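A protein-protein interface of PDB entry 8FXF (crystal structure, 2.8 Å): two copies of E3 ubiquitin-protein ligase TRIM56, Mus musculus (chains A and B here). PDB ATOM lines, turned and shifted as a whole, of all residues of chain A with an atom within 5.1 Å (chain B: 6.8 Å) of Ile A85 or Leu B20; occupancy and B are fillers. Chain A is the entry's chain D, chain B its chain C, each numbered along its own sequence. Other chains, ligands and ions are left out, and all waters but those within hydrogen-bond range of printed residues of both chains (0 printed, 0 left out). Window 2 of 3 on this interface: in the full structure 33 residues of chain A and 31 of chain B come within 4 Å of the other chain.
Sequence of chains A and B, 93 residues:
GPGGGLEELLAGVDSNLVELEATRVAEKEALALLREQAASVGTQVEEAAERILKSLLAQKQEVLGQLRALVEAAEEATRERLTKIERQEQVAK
Printed residues of chain B within 4 Å of Arg A81: Glu B27.
Thr A83 touches none of the printed residues of chain B.
Ile A85 touches two residues of chain B.
Printed residues of chain B within 4 Å of Glu A89: Leu B17 (3.7 Å), Leu B20 (3.5 Å) and Glu B21 (2.6 Å).
Printed residues of chain A within 4 Å of Leu B20: Ile A85 and Glu A89.
Of the printed residues of chain A, Glu B21 touches Glu A89.
The nearest residue of chain B that does not touch Ile A85 is Thr B23 (4.3 Å).
The nearest printed residue of chain B that does not touch Leu A82 is Glu B27 (5.1 Å).
No position is printed for both chains.
Of the 7 pairs that touch across the chains among the printed residues, none has its exchanged pair printed and touching as well.
Leu A82 touches Arg B24 (CD2 to CD, 3.3 Å).
Ile A85 touches Leu B20.
Ile A85 touches Arg B24 (CG2 to NH2, 3.1 Å).
Glu A89 touches Leu B17 (CG to CD2, 3.7 Å).
Glu A89 touches Leu B20 (CG to CD2, 3.5 Å).
OE2 of Glu B21 lies close to OE2 of Glu A89, at 2.6 Å.
The side-chain carboxylate (OE2) of Glu B27 lies within salt-bridge range of the guanidinium group (NE) of Arg A81 (3.6 Å).
The side-chain carboxylate of Glu B21 lies within salt-bridge range of the guanidinium group of Arg B24.
The backbone NH (N) of Ile A85 sits close to the side-chain amide oxygen (OE1) of Gln A88 (3.5 Å).
Of the 11 printed residues of chain B, 5 touch a printed residue of chain A.
Printed residues of chain B that touch a printed residue of chain A: Leu B17, Leu B20, Glu B21, Arg B24 and Glu B27.
Printed residues of chain A that touch a printed residue of chain B: Arg A81, Leu A82, Ile A85 and Glu A89.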
ATOM      1  N   ARG A  81      -4.478 -18.868  -6.494  1.00  0.00           N
ATOM      2  CA  ARG A  81      -3.962 -20.048  -5.813  1.00  0.00           C
ATOM      3  C   ARG A  81      -2.891 -19.699  -4.774  1.00  0.00           C
ATOM      4  O   ARG A  81      -2.554 -20.558  -3.962  1.00  0.00           O
ATOM      5  CB  ARG A  81      -3.372 -21.076  -6.789  1.00  0.00           C
ATOM      6  CG  ARG A  81      -4.363 -22.081  -7.352  1.00  0.00           C
ATOM      7  CD  ARG A  81      -3.898 -23.137  -8.346  1.00  0.00           C
ATOM      8  NE  ARG A  81      -3.705 -22.436  -9.605  1.00  0.00           N
ATOM      9  CZ  ARG A  81      -4.400 -22.651 -10.712  1.00  0.00           C
ATOM     10  NH1 ARG A  81      -5.135 -23.743 -10.814  1.00  0.00           N
ATOM     11  NH2 ARG A  81      -4.323 -21.801 -11.728  1.00  0.00           N
ATOM     12  N   LEU A  82      -2.328 -18.479  -4.809  1.00  0.00           N
ATOM     13  CA  LEU A  82      -1.288 -18.128  -3.845  1.00  0.00           C
ATOM     14  C   LEU A  82      -1.798 -17.136  -2.790  1.00  0.00           C
ATOM     15  O   LEU A  82      -1.284 -17.121  -1.679  1.00  0.00           O
ATOM     16  CB  LEU A  82      -0.003 -17.682  -4.563  1.00  0.00           C
ATOM     17  CG  LEU A  82       0.656 -18.716  -5.488  1.00  0.00           C
ATOM     18  CD1 LEU A  82       2.057 -18.300  -5.929  1.00  0.00           C
ATOM     19  CD2 LEU A  82       0.647 -20.117  -4.883  1.00  0.00           C
ATOM     20  N   THR A  83      -2.837 -16.351  -3.104  1.00  0.00           N
ATOM     21  CA  THR A  83      -3.540 -15.536  -2.120  1.00  0.00           C
ATOM     22  C   THR A  83      -4.256 -16.425  -1.109  1.00  0.00           C
ATOM     23  O   THR A  83      -4.507 -16.015   0.026  1.00  0.00           O
ATOM     24  CB  THR A  83      -4.651 -14.707  -2.774  1.00  0.00           C
ATOM     25  OG1 THR A  83      -4.038 -14.030  -3.868  1.00  0.00           O
ATOM     26  CG2 THR A  83      -5.316 -13.714  -1.843  1.00  0.00           C
ATOM     27  N   LYS A  84      -4.627 -17.627  -1.556  1.00  0.00           N
ATOM     28  CA  LYS A  84      -5.235 -18.592  -0.664  1.00  0.00           C
ATOM     29  C   LYS A  84      -4.146 -19.191   0.218  1.00  0.00           C
ATOM     30  O   LYS A  84      -4.257 -19.093   1.434  1.00  0.00           O
ATOM     31  CB  LYS A  84      -6.009 -19.649  -1.450  1.00  0.00           C
ATOM     32  CG  LYS A  84      -7.413 -19.253  -1.900  1.00  0.00           C
ATOM     33  CD  LYS A  84      -7.970 -20.117  -3.025  1.00  0.00           C
ATOM     34  CE  LYS A  84      -7.448 -21.545  -3.078  1.00  0.00           C
ATOM     35  NZ  LYS A  84      -8.370 -22.525  -2.457  1.00  0.00           N
ATOM     36  N   ILE A  85      -3.095 -19.764  -0.398  1.00  0.00           N
ATOM     37  CA  ILE A  85      -1.991 -20.342   0.355  1.00  0.00           C
ATOM     38  C   ILE A  85      -1.471 -19.342   1.404  1.00  0.00           C
ATOM     39  O   ILE A  85      -1.313 -19.700   2.572  1.00  0.00           O
ATOM     40  CB  ILE A  85      -0.911 -20.957  -0.563  1.00  0.00           C
ATOM     41  CG1 ILE A  85      -1.432 -22.214  -1.271  1.00  0.00           C
ATOM     42  CG2 ILE A  85       0.347 -21.260   0.238  1.00  0.00           C
ATOM     43  CD1 ILE A  85      -0.434 -22.939  -2.189  1.00  0.00           C
ATOM     44  N   GLU A  86      -1.324 -18.062   1.035  1.00  0.00           N
ATOM     45  CA  GLU A  86      -0.794 -17.042   1.937  1.00  0.00           C
ATOM     46  C   GLU A  86      -1.658 -16.849   3.190  1.00  0.00           C
ATOM     47  O   GLU A  86      -1.135 -16.550   4.273  1.00  0.00           O
ATOM     48  CB  GLU A  86      -0.647 -15.711   1.202  1.00  0.00           C
ATOM     49  CG  GLU A  86       0.493 -14.873   1.740  1.00  0.00           C
ATOM     50  CD  GLU A  86       1.023 -13.844   0.761  1.00  0.00           C
ATOM     51  OE1 GLU A  86       1.071 -14.149  -0.447  1.00  0.00           O
ATOM     52  OE2 GLU A  86       1.423 -12.761   1.213  1.00  0.00           O
ATOM     53  N   ARG A  87      -2.980 -17.013   3.029  1.00  0.00           N
ATOM     54  CA  ARG A  87      -3.953 -16.881   4.107  1.00  0.00           C
ATOM     55  C   ARG A  87      -3.929 -18.105   5.033  1.00  0.00           C
ATOM     56  O   ARG A  87      -3.907 -17.969   6.265  1.00  0.00           O
ATOM     57  CB  ARG A  87      -5.353 -16.620   3.539  1.00  0.00           C
ATOM     58  N   GLN A  88      -3.940 -19.303   4.428  1.00  0.00           N
ATOM     59  CA  GLN A  88      -3.929 -20.563   5.156  1.00  0.00           C
ATOM     60  C   GLN A  88      -2.614 -20.740   5.916  1.00  0.00           C
ATOM     61  O   GLN A  88      -2.514 -21.599   6.789  1.00  0.00           O
ATOM     62  CB  GLN A  88      -4.049 -21.767   4.220  1.00  0.00           C
ATOM     63  CG  GLN A  88      -4.970 -21.575   3.025  1.00  0.00           C
ATOM     64  CD  GLN A  88      -4.865 -22.766   2.102  1.00  0.00           C
ATOM     65  OE1 GLN A  88      -4.335 -22.686   0.993  1.00  0.00           O
ATOM     66  NE2 GLN A  88      -5.330 -23.907   2.582  1.00  0.00           N
ATOM     67  N   GLU A  89      -1.586 -19.966   5.529  1.00  0.00           N
ATOM     68  CA  GLU A  89      -0.309 -19.958   6.232  1.00  0.00           C
ATOM     69  C   GLU A  89      -0.343 -19.047   7.462  1.00  0.00           C
ATOM     70  O   GLU A  89       0.355 -19.294   8.444  1.00  0.00           O
ATOM     71  CB  GLU A  89       0.838 -19.672   5.263  1.00  0.00           C
ATOM     72  CG  GLU A  89       1.283 -20.937   4.560  1.00  0.00           C
ATOM     73  CD  GLU A  89       2.380 -20.717   3.546  1.00  0.00           C
ATOM     74  OE1 GLU A  89       2.568 -19.560   3.146  1.00  0.00           O
ATOM     75  OE2 GLU A  89       3.053 -21.698   3.194  1.00  0.00           O
ATOM     76  N   ASN B  16       4.179 -29.455   9.268  1.00  0.00           N
ATOM     77  CA  ASN B  16       2.965 -28.650   9.346  1.00  0.00           C
ATOM     78  C   ASN B  16       2.648 -28.096   7.945  1.00  0.00           C
ATOM     79  O   ASN B  16       1.583 -28.379   7.369  1.00  0.00           O
ATOM     80  CB  ASN B  16       3.119 -27.580  10.446  1.00  0.00           C
ATOM     81  CG  ASN B  16       1.825 -27.010  11.012  1.00  0.00           C
ATOM     82  OD1 ASN B  16       1.635 -25.794  11.077  1.00  0.00           O
ATOM     83  ND2 ASN B  16       0.931 -27.878  11.457  1.00  0.00           N
ATOM     84  N   LEU B  17       3.623 -27.330   7.405  1.00  0.00           N
ATOM     85  CA  LEU B  17       3.501 -26.427   6.264  1.00  0.00           C
ATOM     86  C   LEU B  17       4.285 -26.948   5.048  1.00  0.00           C
ATOM     87  O   LEU B  17       4.408 -26.231   4.057  1.00  0.00           O
ATOM     88  CB  LEU B  17       4.038 -25.039   6.669  1.00  0.00           C
ATOM     89  CG  LEU B  17       3.106 -24.017   7.339  1.00  0.00           C
ATOM     90  CD1 LEU B  17       3.761 -22.636   7.412  1.00  0.00           C
ATOM     91  CD2 LEU B  17       1.759 -23.909   6.635  1.00  0.00           C
ATOM     92  N   VAL B  18       4.797 -28.190   5.112  1.00  0.00           N
ATOM     93  CA  VAL B  18       5.737 -28.763   4.149  1.00  0.00           C
ATOM     94  C   VAL B  18       5.062 -29.133   2.831  1.00  0.00           C
ATOM     95  O   VAL B  18       5.726 -29.158   1.798  1.00  0.00           O
ATOM     96  CB  VAL B  18       6.485 -29.991   4.711  1.00  0.00           C
ATOM     97  CG1 VAL B  18       7.016 -30.943   3.632  1.00  0.00           C
ATOM     98  CG2 VAL B  18       7.584 -29.579   5.680  1.00  0.00           C
ATOM     99  N   GLU B  19       3.778 -29.497   2.874  1.00  0.00           N
ATOM    100  CA  GLU B  19       3.086 -29.791   1.633  1.00  0.00           C
ATOM    101  C   GLU B  19       2.220 -28.586   1.255  1.00  0.00           C
ATOM    102  O   GLU B  19       1.610 -28.596   0.191  1.00  0.00           O
ATOM    103  CB  GLU B  19       2.395 -31.163   1.695  1.00  0.00           C
ATOM    104  CG  GLU B  19       2.434 -31.950   0.383  1.00  0.00           C
ATOM    105  CD  GLU B  19       1.253 -31.884  -0.584  1.00  0.00           C
ATOM    106  OE1 GLU B  19       0.116 -31.570  -0.150  1.00  0.00           O
ATOM    107  OE2 GLU B  19       1.469 -32.150  -1.786  1.00  0.00           O
ATOM    108  N   LEU B  20       2.186 -27.542   2.108  1.00  0.00           N
ATOM    109  CA  LEU B  20       1.615 -26.251   1.727  1.00  0.00           C
ATOM    110  C   LEU B  20       2.657 -25.472   0.912  1.00  0.00           C
ATOM    111  O   LEU B  20       2.323 -24.458   0.282  1.00  0.00           O
ATOM    112  CB  LEU B  20       1.097 -25.491   2.964  1.00  0.00           C
ATOM    113  CG  LEU B  20      -0.074 -24.496   2.793  1.00  0.00           C
ATOM    114  CD1 LEU B  20      -1.316 -25.091   2.106  1.00  0.00           C
ATOM    115  CD2 LEU B  20      -0.494 -23.885   4.135  1.00  0.00           C
ATOM    116  N   GLU B  21       3.892 -26.023   0.873  1.00  0.00           N
ATOM    117  CA  GLU B  21       5.043 -25.525   0.123  1.00  0.00           C
ATOM    118  C   GLU B  21       5.419 -26.448  -1.032  1.00  0.00           C
ATOM    119  O   GLU B  21       5.716 -25.943  -2.112  1.00  0.00           O
ATOM    120  CB  GLU B  21       6.277 -25.340   1.008  1.00  0.00           C
ATOM    121  CG  GLU B  21       6.095 -24.260   2.056  1.00  0.00           C
ATOM    122  CD  GLU B  21       5.815 -22.864   1.524  1.00  0.00           C
ATOM    123  OE1 GLU B  21       5.937 -22.655   0.293  1.00  0.00           O
ATOM    124  OE2 GLU B  21       5.453 -21.991   2.340  1.00  0.00           O
ATOM    125  N   ALA B  22       5.438 -27.775  -0.797  1.00  0.00           N
ATOM    126  CA  ALA B  22       5.806 -28.768  -1.811  1.00  0.00           C
ATOM    127  C   ALA B  22       4.845 -28.679  -2.996  1.00  0.00           C
ATOM    128  O   ALA B  22       5.156 -29.131  -4.100  1.00  0.00           O
ATOM    129  CB  ALA B  22       5.821 -30.166  -1.229  1.00  0.00           C
ATOM    130  N   THR B  23       3.685 -28.077  -2.703  1.00  0.00           N
ATOM    131  CA  THR B  23       2.579 -27.806  -3.603  1.00  0.00           C
ATOM    132  C   THR B  23       2.861 -26.506  -4.353  1.00  0.00           C
ATOM    133  O   THR B  23       2.748 -26.500  -5.571  1.00  0.00           O
ATOM    134  CB  THR B  23       1.245 -27.923  -2.848  1.00  0.00           C
ATOM    135  OG1 THR B  23       0.903 -29.316  -2.849  1.00  0.00           O
ATOM    136  CG2 THR B  23       0.128 -27.038  -3.370  1.00  0.00           C
ATOM    137  N   ARG B  24       3.279 -25.436  -3.656  1.00  0.00           N
ATOM    138  CA  ARG B  24       3.558 -24.201  -4.375  1.00  0.00           C
ATOM    139  C   ARG B  24       4.767 -24.352  -5.319  1.00  0.00           C
ATOM    140  O   ARG B  24       4.834 -23.709  -6.365  1.00  0.00           O
ATOM    141  CB  ARG B  24       3.510 -22.971  -3.465  1.00  0.00           C
ATOM    142  CG  ARG B  24       3.623 -21.683  -4.266  1.00  0.00           C
ATOM    143  CD  ARG B  24       3.639 -20.402  -3.464  1.00  0.00           C
ATOM    144  NE  ARG B  24       4.698 -20.313  -2.472  1.00  0.00           N
ATOM    145  CZ  ARG B  24       4.470 -20.286  -1.167  1.00  0.00           C
ATOM    146  NH1 ARG B  24       5.453 -20.038  -0.321  1.00  0.00           N
ATOM    147  NH2 ARG B  24       3.243 -20.485  -0.716  1.00  0.00           N
ATOM    148  N   VAL B  25       5.653 -25.308  -5.021  1.00  0.00           N
ATOM    149  CA  VAL B  25       6.810 -25.644  -5.848  1.00  0.00           C
ATOM    150  C   VAL B  25       6.484 -26.656  -6.963  1.00  0.00           C
ATOM    151  O   VAL B  25       7.347 -26.998  -7.775  1.00  0.00           O
ATOM    152  CB  VAL B  25       7.977 -26.086  -4.935  1.00  0.00           C
ATOM    153  CG1 VAL B  25       8.933 -27.094  -5.579  1.00  0.00           C
ATOM    154  CG2 VAL B  25       8.712 -24.880  -4.352  1.00  0.00           C
ATOM    155  N   GLU B  27       3.507 -25.833  -8.423  1.00  0.00           N
ATOM    156  CA  GLU B  27       2.717 -24.781  -9.046  1.00  0.00           C
ATOM    157  C   GLU B  27       3.630 -23.791  -9.754  1.00  0.00           C
ATOM    158  O   GLU B  27       3.407 -23.492 -10.927  1.00  0.00           O
ATOM    159  CB  GLU B  27       1.891 -23.981  -8.032  1.00  0.00           C
ATOM    160  CG  GLU B  27       0.750 -24.745  -7.366  1.00  0.00           C
ATOM    161  CD  GLU B  27      -0.260 -25.556  -8.172  1.00  0.00           C
ATOM    162  OE1 GLU B  27       0.027 -26.779  -8.478  1.00  0.00           O
ATOM    163  OE2 GLU B  27      -1.352 -24.978  -8.459  1.00  0.00           O
